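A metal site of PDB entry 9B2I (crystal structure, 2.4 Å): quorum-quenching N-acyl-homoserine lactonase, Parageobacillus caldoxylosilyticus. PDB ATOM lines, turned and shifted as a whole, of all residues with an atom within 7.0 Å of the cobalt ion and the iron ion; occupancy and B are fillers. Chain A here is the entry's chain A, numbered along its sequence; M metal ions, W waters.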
ATOM      1  N   MET A  34     -29.088  13.112  -5.366  1.00  0.00           N
ATOM      2  CA  MET A  34     -29.865  13.594  -4.230  1.00  0.00           C
ATOM      3  C   MET A  34     -31.295  13.843  -4.692  1.00  0.00           C
ATOM      4  O   MET A  34     -31.530  14.115  -5.863  1.00  0.00           O
ATOM      5  CB  MET A  34     -29.259  14.876  -3.659  1.00  0.00           C
ATOM      6  CG  MET A  34     -29.869  15.332  -2.345  1.00  0.00           C
ATOM      7  SD  MET A  34     -28.991  16.746  -1.629  1.00  0.00           S
ATOM      8  CE  MET A  34     -27.530  15.898  -1.023  1.00  0.00           C
ATOM      9  N   PHE A  62     -31.373  14.736  -8.559  1.00  0.00           N
ATOM     10  CA  PHE A  62     -30.399  15.579  -9.219  1.00  0.00           C
ATOM     11  C   PHE A  62     -28.991  15.100  -8.895  1.00  0.00           C
ATOM     12  O   PHE A  62     -28.757  14.503  -7.846  1.00  0.00           O
ATOM     13  CB  PHE A  62     -30.595  17.046  -8.838  1.00  0.00           C
ATOM     14  CG  PHE A  62     -30.604  17.348  -7.343  1.00  0.00           C
ATOM     15  CD1 PHE A  62     -31.791  17.306  -6.613  1.00  0.00           C
ATOM     16  CD2 PHE A  62     -29.433  17.691  -6.671  1.00  0.00           C
ATOM     17  CE1 PHE A  62     -31.799  17.599  -5.256  1.00  0.00           C
ATOM     18  CE2 PHE A  62     -29.452  17.970  -5.318  1.00  0.00           C
ATOM     19  CZ  PHE A  62     -30.631  17.923  -4.616  1.00  0.00           C
ATOM     20  N   PRO A  63     -28.006  15.341  -9.796  1.00  0.00           N
ATOM     21  CA  PRO A  63     -26.629  14.924  -9.564  1.00  0.00           C
ATOM     22  C   PRO A  63     -25.832  15.846  -8.661  1.00  0.00           C
ATOM     23  O   PRO A  63     -25.891  17.070  -8.780  1.00  0.00           O
ATOM     24  CB  PRO A  63     -26.051  14.897 -10.995  1.00  0.00           C
ATOM     25  CG  PRO A  63     -26.807  16.004 -11.711  1.00  0.00           C
ATOM     26  CD  PRO A  63     -28.203  15.991 -11.100  1.00  0.00           C
ATOM     27  N   ILE A  64     -25.094  15.235  -7.733  1.00  0.00           N
ATOM     28  CA  ILE A  64     -24.018  15.899  -7.013  1.00  0.00           C
ATOM     29  C   ILE A  64     -22.717  15.594  -7.752  1.00  0.00           C
ATOM     30  O   ILE A  64     -22.432  14.433  -8.033  1.00  0.00           O
ATOM     31  CB  ILE A  64     -23.948  15.397  -5.557  1.00  0.00           C
ATOM     32  CG1 ILE A  64     -25.326  15.366  -4.902  1.00  0.00           C
ATOM     33  CG2 ILE A  64     -22.933  16.203  -4.743  1.00  0.00           C
ATOM     34  CD1 ILE A  64     -26.077  16.688  -4.975  1.00  0.00           C
ATOM     35  N   ASP A  79     -15.605  22.330  -5.406  1.00  0.00           N
ATOM     36  CA  ASP A  79     -16.606  21.622  -4.616  1.00  0.00           C
ATOM     37  C   ASP A  79     -16.032  20.284  -4.157  1.00  0.00           C
ATOM     38  O   ASP A  79     -14.967  19.877  -4.607  1.00  0.00           O
ATOM     39  CB  ASP A  79     -17.929  21.508  -5.370  1.00  0.00           C
ATOM     40  CG  ASP A  79     -18.801  22.753  -5.329  1.00  0.00           C
ATOM     41  OD1 ASP A  79     -18.457  23.697  -4.600  1.00  0.00           O
ATOM     42  OD2 ASP A  79     -19.828  22.764  -6.044  1.00  0.00           O
ATOM     43  N   SER A 131     -17.746  26.449  -3.552  1.00  0.00           N
ATOM     44  CA  SER A 131     -18.765  27.321  -4.104  1.00  0.00           C
ATOM     45  C   SER A 131     -19.559  27.932  -2.953  1.00  0.00           C
ATOM     46  O   SER A 131     -19.826  29.132  -2.937  1.00  0.00           O
ATOM     47  CB  SER A 131     -19.664  26.582  -5.059  1.00  0.00           C
ATOM     48  OG  SER A 131     -20.409  25.574  -4.386  1.00  0.00           O
ATOM     49  N   HIS A 132     -19.932  27.077  -2.000  1.00  0.00           N
ATOM     50  CA  HIS A 132     -20.544  27.466  -0.740  1.00  0.00           C
ATOM     51  C   HIS A 132     -20.381  26.292   0.218  1.00  0.00           C
ATOM     52  O   HIS A 132     -19.696  25.328  -0.112  1.00  0.00           O
ATOM     53  CB  HIS A 132     -21.992  27.934  -0.956  1.00  0.00           C
ATOM     54  CG  HIS A 132     -22.892  26.931  -1.617  1.00  0.00           C
ATOM     55  ND1 HIS A 132     -22.547  26.230  -2.746  1.00  0.00           N
ATOM     56  CD2 HIS A 132     -24.138  26.561  -1.305  1.00  0.00           C
ATOM     57  CE1 HIS A 132     -23.549  25.441  -3.095  1.00  0.00           C
ATOM     58  NE2 HIS A 132     -24.528  25.621  -2.228  1.00  0.00           N
ATOM     59  N   LEU A 133     -20.988  26.370   1.401  1.00  0.00           N
ATOM     60  CA  LEU A 133     -20.690  25.399   2.440  1.00  0.00           C
ATOM     61  C   LEU A 133     -21.919  24.542   2.767  1.00  0.00           C
ATOM     62  O   LEU A 133     -22.045  24.029   3.877  1.00  0.00           O
ATOM     63  CB  LEU A 133     -20.163  26.136   3.675  1.00  0.00           C
ATOM     64  CG  LEU A 133     -18.823  26.844   3.477  1.00  0.00           C
ATOM     65  CD1 LEU A 133     -18.399  27.561   4.752  1.00  0.00           C
ATOM     66  CD2 LEU A 133     -17.744  25.875   3.026  1.00  0.00           C
ATOM     67  N   HIS A 134     -22.790  24.365   1.771  1.00  0.00           N
ATOM     68  CA  HIS A 134     -23.909  23.455   1.888  1.00  0.00           C
ATOM     69  C   HIS A 134     -23.395  22.022   1.977  1.00  0.00           C
ATOM     70  O   HIS A 134     -22.257  21.736   1.588  1.00  0.00           O
ATOM     71  CB  HIS A 134     -24.889  23.638   0.724  1.00  0.00           C
ATOM     72  CG  HIS A 134     -25.854  24.754   0.904  1.00  0.00           C
ATOM     73  ND1 HIS A 134     -26.679  25.199  -0.101  1.00  0.00           N
ATOM     74  CD2 HIS A 134     -26.164  25.492   1.986  1.00  0.00           C
ATOM     75  CE1 HIS A 134     -27.446  26.185   0.361  1.00  0.00           C
ATOM     76  NE2 HIS A 134     -27.138  26.382   1.630  1.00  0.00           N
ATOM     77  N   LEU A 135     -24.256  21.124   2.458  1.00  0.00           N
ATOM     78  CA  LEU A 135     -23.887  19.761   2.789  1.00  0.00           C
ATOM     79  C   LEU A 135     -23.409  19.006   1.555  1.00  0.00           C
ATOM     80  O   LEU A 135     -22.573  18.111   1.656  1.00  0.00           O
ATOM     81  CB  LEU A 135     -25.075  19.062   3.446  1.00  0.00           C
ATOM     82  CG  LEU A 135     -26.303  18.832   2.569  1.00  0.00           C
ATOM     83  CD1 LEU A 135     -27.375  18.091   3.354  1.00  0.00           C
ATOM     84  CD2 LEU A 135     -26.875  20.125   2.018  1.00  0.00           C
ATOM     85  N   ASP A 136     -23.927  19.387   0.375  1.00  0.00           N
ATOM     86  CA  ASP A 136     -23.678  18.643  -0.845  1.00  0.00           C
ATOM     87  C   ASP A 136     -22.573  19.307  -1.665  1.00  0.00           C
ATOM     88  O   ASP A 136     -22.434  19.042  -2.858  1.00  0.00           O
ATOM     89  CB  ASP A 136     -24.938  18.506  -1.673  1.00  0.00           C
ATOM     90  CG  ASP A 136     -25.616  19.818  -2.038  1.00  0.00           C
ATOM     91  OD1 ASP A 136     -25.819  20.643  -1.118  1.00  0.00           O
ATOM     92  OD2 ASP A 136     -25.937  20.013  -3.230  1.00  0.00           O
ATOM     93  N   HIS A 137     -21.782  20.172  -1.016  1.00  0.00           N
ATOM     94  CA  HIS A 137     -20.710  20.872  -1.701  1.00  0.00           C
ATOM     95  C   HIS A 137     -19.458  20.937  -0.832  1.00  0.00           C
ATOM     96  O   HIS A 137     -18.337  20.974  -1.350  1.00  0.00           O
ATOM     97  CB  HIS A 137     -21.153  22.276  -2.113  1.00  0.00           C
ATOM     98  CG  HIS A 137     -22.252  22.301  -3.122  1.00  0.00           C
ATOM     99  ND1 HIS A 137     -22.033  22.418  -4.472  1.00  0.00           N
ATOM    100  CD2 HIS A 137     -23.582  22.223  -2.969  1.00  0.00           C
ATOM    101  CE1 HIS A 137     -23.197  22.405  -5.116  1.00  0.00           C
ATOM    102  NE2 HIS A 137     -24.154  22.289  -4.213  1.00  0.00           N
ATOM    103  N   GLU A 155     -20.020  33.290   3.702  1.00  0.00           N
ATOM    104  CA  GLU A 155     -20.465  31.911   3.794  1.00  0.00           C
ATOM    105  C   GLU A 155     -19.769  31.239   4.967  1.00  0.00           C
ATOM    106  O   GLU A 155     -20.384  30.486   5.730  1.00  0.00           O
ATOM    107  CB  GLU A 155     -20.169  31.167   2.491  1.00  0.00           C
ATOM    108  CG  GLU A 155     -20.719  29.743   2.469  1.00  0.00           C
ATOM    109  CD  GLU A 155     -22.225  29.649   2.316  1.00  0.00           C
ATOM    110  OE1 GLU A 155     -22.876  30.705   2.139  1.00  0.00           O
ATOM    111  OE2 GLU A 155     -22.758  28.521   2.392  1.00  0.00           O
ATOM    112  N   ALA A 171     -29.018  22.645   5.950  1.00  0.00           N
ATOM    113  CA  ALA A 171     -28.082  22.633   4.828  1.00  0.00           C
ATOM    114  C   ALA A 171     -26.633  22.660   5.314  1.00  0.00           C
ATOM    115  O   ALA A 171     -25.727  22.392   4.544  1.00  0.00           O
ATOM    116  CB  ALA A 171     -28.381  23.790   3.904  1.00  0.00           C
ATOM    117  N   TYR A 172     -26.443  22.974   6.600  1.00  0.00           N
ATOM    118  CA  TYR A 172     -25.097  23.087   7.149  1.00  0.00           C
ATOM    119  C   TYR A 172     -24.911  22.015   8.218  1.00  0.00           C
ATOM    120  O   TYR A 172     -25.659  21.966   9.196  1.00  0.00           O
ATOM    121  CB  TYR A 172     -24.867  24.513   7.654  1.00  0.00           C
ATOM    122  CG  TYR A 172     -24.907  25.570   6.551  1.00  0.00           C
ATOM    123  CD1 TYR A 172     -23.768  25.905   5.837  1.00  0.00           C
ATOM    124  CD2 TYR A 172     -26.087  26.230   6.229  1.00  0.00           C
ATOM    125  CE1 TYR A 172     -23.798  26.853   4.833  1.00  0.00           C
ATOM    126  CE2 TYR A 172     -26.132  27.182   5.230  1.00  0.00           C
ATOM    127  CZ  TYR A 172     -24.988  27.503   4.525  1.00  0.00           C
ATOM    128  OH  TYR A 172     -25.019  28.441   3.540  1.00  0.00           O
ATOM    129  N   HIS A 212     -28.161  32.481  -3.457  1.00  0.00           N
ATOM    130  CA  HIS A 212     -28.586  31.155  -3.028  1.00  0.00           C
ATOM    131  C   HIS A 212     -28.212  30.976  -1.564  1.00  0.00           C
ATOM    132  O   HIS A 212     -29.024  30.515  -0.764  1.00  0.00           O
ATOM    133  CB  HIS A 212     -27.963  30.084  -3.931  1.00  0.00           C
ATOM    134  CG  HIS A 212     -28.064  28.699  -3.409  1.00  0.00           C
ATOM    135  ND1 HIS A 212     -29.228  27.957  -3.459  1.00  0.00           N
ATOM    136  CD2 HIS A 212     -27.156  27.909  -2.817  1.00  0.00           C
ATOM    137  CE1 HIS A 212     -29.013  26.763  -2.920  1.00  0.00           C
ATOM    138  NE2 HIS A 212     -27.761  26.713  -2.524  1.00  0.00           N
ATOM    139  N   ALA A 213     -26.968  31.337  -1.236  1.00  0.00           N
ATOM    140  CA  ALA A 213     -26.472  31.273   0.132  1.00  0.00           C
ATOM    141  C   ALA A 213     -25.789  32.596   0.496  1.00  0.00           C
ATOM    142  O   ALA A 213     -25.860  33.563  -0.259  1.00  0.00           O
ATOM    143  CB  ALA A 213     -25.528  30.101   0.289  1.00  0.00           C
ATOM    144  N   MET A 216     -21.445  33.038  -2.464  1.00  0.00           N
ATOM    145  CA  MET A 216     -21.267  32.070  -3.530  1.00  0.00           C
ATOM    146  C   MET A 216     -20.010  32.394  -4.325  1.00  0.00           C
ATOM    147  O   MET A 216     -19.749  33.556  -4.637  1.00  0.00           O
ATOM    148  CB  MET A 216     -22.472  32.085  -4.477  1.00  0.00           C
ATOM    149  CG  MET A 216     -23.810  31.895  -3.785  1.00  0.00           C
ATOM    150  SD  MET A 216     -24.031  30.233  -3.128  1.00  0.00           S
ATOM    151  CE  MET A 216     -23.973  29.274  -4.645  1.00  0.00           C
ATOM    152  N   SER A 233     -22.307  26.416 -10.065  1.00  0.00           N
ATOM    153  CA  SER A 233     -22.766  25.740  -8.860  1.00  0.00           C
ATOM    154  C   SER A 233     -24.219  26.115  -8.592  1.00  0.00           C
ATOM    155  O   SER A 233     -25.014  26.234  -9.521  1.00  0.00           O
ATOM    156  CB  SER A 233     -21.867  26.058  -7.689  1.00  0.00           C
ATOM    157  OG  SER A 233     -22.308  25.390  -6.508  1.00  0.00           O
ATOM    158  N   ASP A 234     -24.551  26.344  -7.321  1.00  0.00           N
ATOM    159  CA  ASP A 234     -25.932  26.536  -6.907  1.00  0.00           C
ATOM    160  C   ASP A 234     -26.390  27.966  -7.178  1.00  0.00           C
ATOM    161  O   ASP A 234     -27.501  28.336  -6.821  1.00  0.00           O
ATOM    162  CB  ASP A 234     -26.149  26.174  -5.453  1.00  0.00           C
ATOM    163  CG  ASP A 234     -26.189  24.686  -5.143  1.00  0.00           C
ATOM    164  OD1 ASP A 234     -26.011  23.884  -6.078  1.00  0.00           O
ATOM    165  OD2 ASP A 234     -26.409  24.338  -3.959  1.00  0.00           O
ATOM    166  N   ALA A 235     -25.539  28.784  -7.803  1.00  0.00           N
ATOM    167  CA  ALA A 235     -25.957  30.084  -8.293  1.00  0.00           C
ATOM    168  C   ALA A 235     -27.052  29.870  -9.338  1.00  0.00           C
ATOM    169  O   ALA A 235     -27.953  30.687  -9.490  1.00  0.00           O
ATOM    170  CB  ALA A 235     -24.789  30.854  -8.850  1.00  0.00           C
ATOM    171  N   TYR A 237     -29.253  26.388 -10.375  1.00  0.00           N
ATOM    172  CA  TYR A 237     -29.532  24.974 -10.156  1.00  0.00           C
ATOM    173  C   TYR A 237     -29.588  24.232 -11.484  1.00  0.00           C
ATOM    174  O   TYR A 237     -28.901  23.234 -11.663  1.00  0.00           O
ATOM    175  CB  TYR A 237     -30.862  24.814  -9.405  1.00  0.00           C
ATOM    176  CG  TYR A 237     -30.812  24.763  -7.876  1.00  0.00           C
ATOM    177  CD1 TYR A 237     -29.683  24.331  -7.193  1.00  0.00           C
ATOM    178  CD2 TYR A 237     -31.924  25.112  -7.123  1.00  0.00           C
ATOM    179  CE1 TYR A 237     -29.654  24.266  -5.807  1.00  0.00           C
ATOM    180  CE2 TYR A 237     -31.914  25.057  -5.745  1.00  0.00           C
ATOM    181  CZ  TYR A 237     -30.770  24.641  -5.082  1.00  0.00           C
ATOM    182  OH  TYR A 237     -30.761  24.583  -3.721  1.00  0.00           O
ATOM    183  N   ILE A 251     -34.795  27.416  -1.754  1.00  0.00           N
ATOM    184  CA  ILE A 251     -33.580  27.583  -0.966  1.00  0.00           C
ATOM    185  C   ILE A 251     -32.887  28.850  -1.447  1.00  0.00           C
ATOM    186  O   ILE A 251     -32.346  28.883  -2.548  1.00  0.00           O
ATOM    187  CB  ILE A 251     -32.640  26.366  -1.082  1.00  0.00           C
ATOM    188  CG1 ILE A 251     -33.330  25.060  -0.659  1.00  0.00           C
ATOM    189  CG2 ILE A 251     -31.365  26.596  -0.288  1.00  0.00           C
ATOM    190  CD1 ILE A 251     -32.373  23.898  -0.469  1.00  0.00           C
ATOM    191  N   GLY A 279     -25.291  23.599 -11.360  1.00  0.00           N
ATOM    192  CA  GLY A 279     -24.853  22.844 -10.194  1.00  0.00           C
ATOM    193  C   GLY A 279     -25.531  21.481 -10.101  1.00  0.00           C
ATOM    194  O   GLY A 279     -24.917  20.524  -9.624  1.00  0.00           O
ATOM    195  N   HIS A 280     -26.775  21.394 -10.568  1.00  0.00           N
ATOM    196  CA  HIS A 280     -27.581  20.199 -10.338  1.00  0.00           C
ATOM    197  C   HIS A 280     -28.585  19.983 -11.477  1.00  0.00           C
ATOM    198  O   HIS A 280     -29.758  19.751 -11.225  1.00  0.00           O
ATOM    199  CB  HIS A 280     -28.348  20.326  -9.015  1.00  0.00           C
ATOM    200  CG  HIS A 280     -27.476  20.501  -7.814  1.00  0.00           C
ATOM    201  ND1 HIS A 280     -26.448  19.641  -7.481  1.00  0.00           N
ATOM    202  CD2 HIS A 280     -27.510  21.429  -6.849  1.00  0.00           C
ATOM    203  CE1 HIS A 280     -25.879  20.063  -6.358  1.00  0.00           C
ATOM    204  NE2 HIS A 280     -26.513  21.148  -5.955  1.00  0.00           N
HETATM  205 CO    CO M   1     -26.593  24.973  -2.113  1.00  0.00          CO
HETATM  206 FE    FE M   2     -26.167  22.064  -4.127  1.00  0.00          FE
HETATM  207  O   HOH W   1     -26.611  22.704  -1.985  1.00  0.00           O
HETATM  208  O   HOH W   2     -28.281  22.186  -3.844  1.00  0.00           O
HETATM  209  O   HOH W   3     -28.436  24.084  -2.358  1.00  0.00           O
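The iron ion is bound by a ring nitrogen (NE2) of His 137 (2.0 Å), a ring nitrogen (NE2) of His 280 (2.1 Å), water W2 (2.1 Å), the side-chain carboxylate (OD2) of Asp 136 (2.3 Å), water W1 (2.3 Å) and the side-chain carboxylate (OD2) of Asp 234 (2.3 Å). The iron ion has six donor atoms within binding distance. Slightly farther from the iron ion lies OD1 of Asp 234 (2.7 Å).
The cobalt ion is bound by OD2 of Asp 234, ND1 of His 134, water W3, NE2 of His 212, NE2 of His 132 and water W1.
The backbone carbonyl oxygen of Tyr 237 is in hydrogen-bond range of the backbone NH of His 280. A ring nitrogen (ND1) of His 212 sits at hydrogen-bond distance from the backbone carbonyl oxygen of Ile 251 (3.4 Å). ND1 of His 132 is in hydrogen-bond range of OG of Ser 131 (2.8 Å). The side-chain carboxylate of Asp 79 lies within hydrogen-bond range of a ring nitrogen (ND1) of His 137 (2.7 Å). ND1 of His 280 is in hydrogen-bond range of O of Pro 63 (2.9 Å).
Within 4 Å of the cobalt ion: His 132, His 134, His 212 and Asp 234. The nearest printed residue that does not touch the cobalt ion is His 137 (4.2 Å).
Four residues have an atom within 4 Å of the iron ion: Asp 136, His 137, Asp 234 and His 280. The nearest printed residue that does not touch the iron ion is His 132 (4.4 Å).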
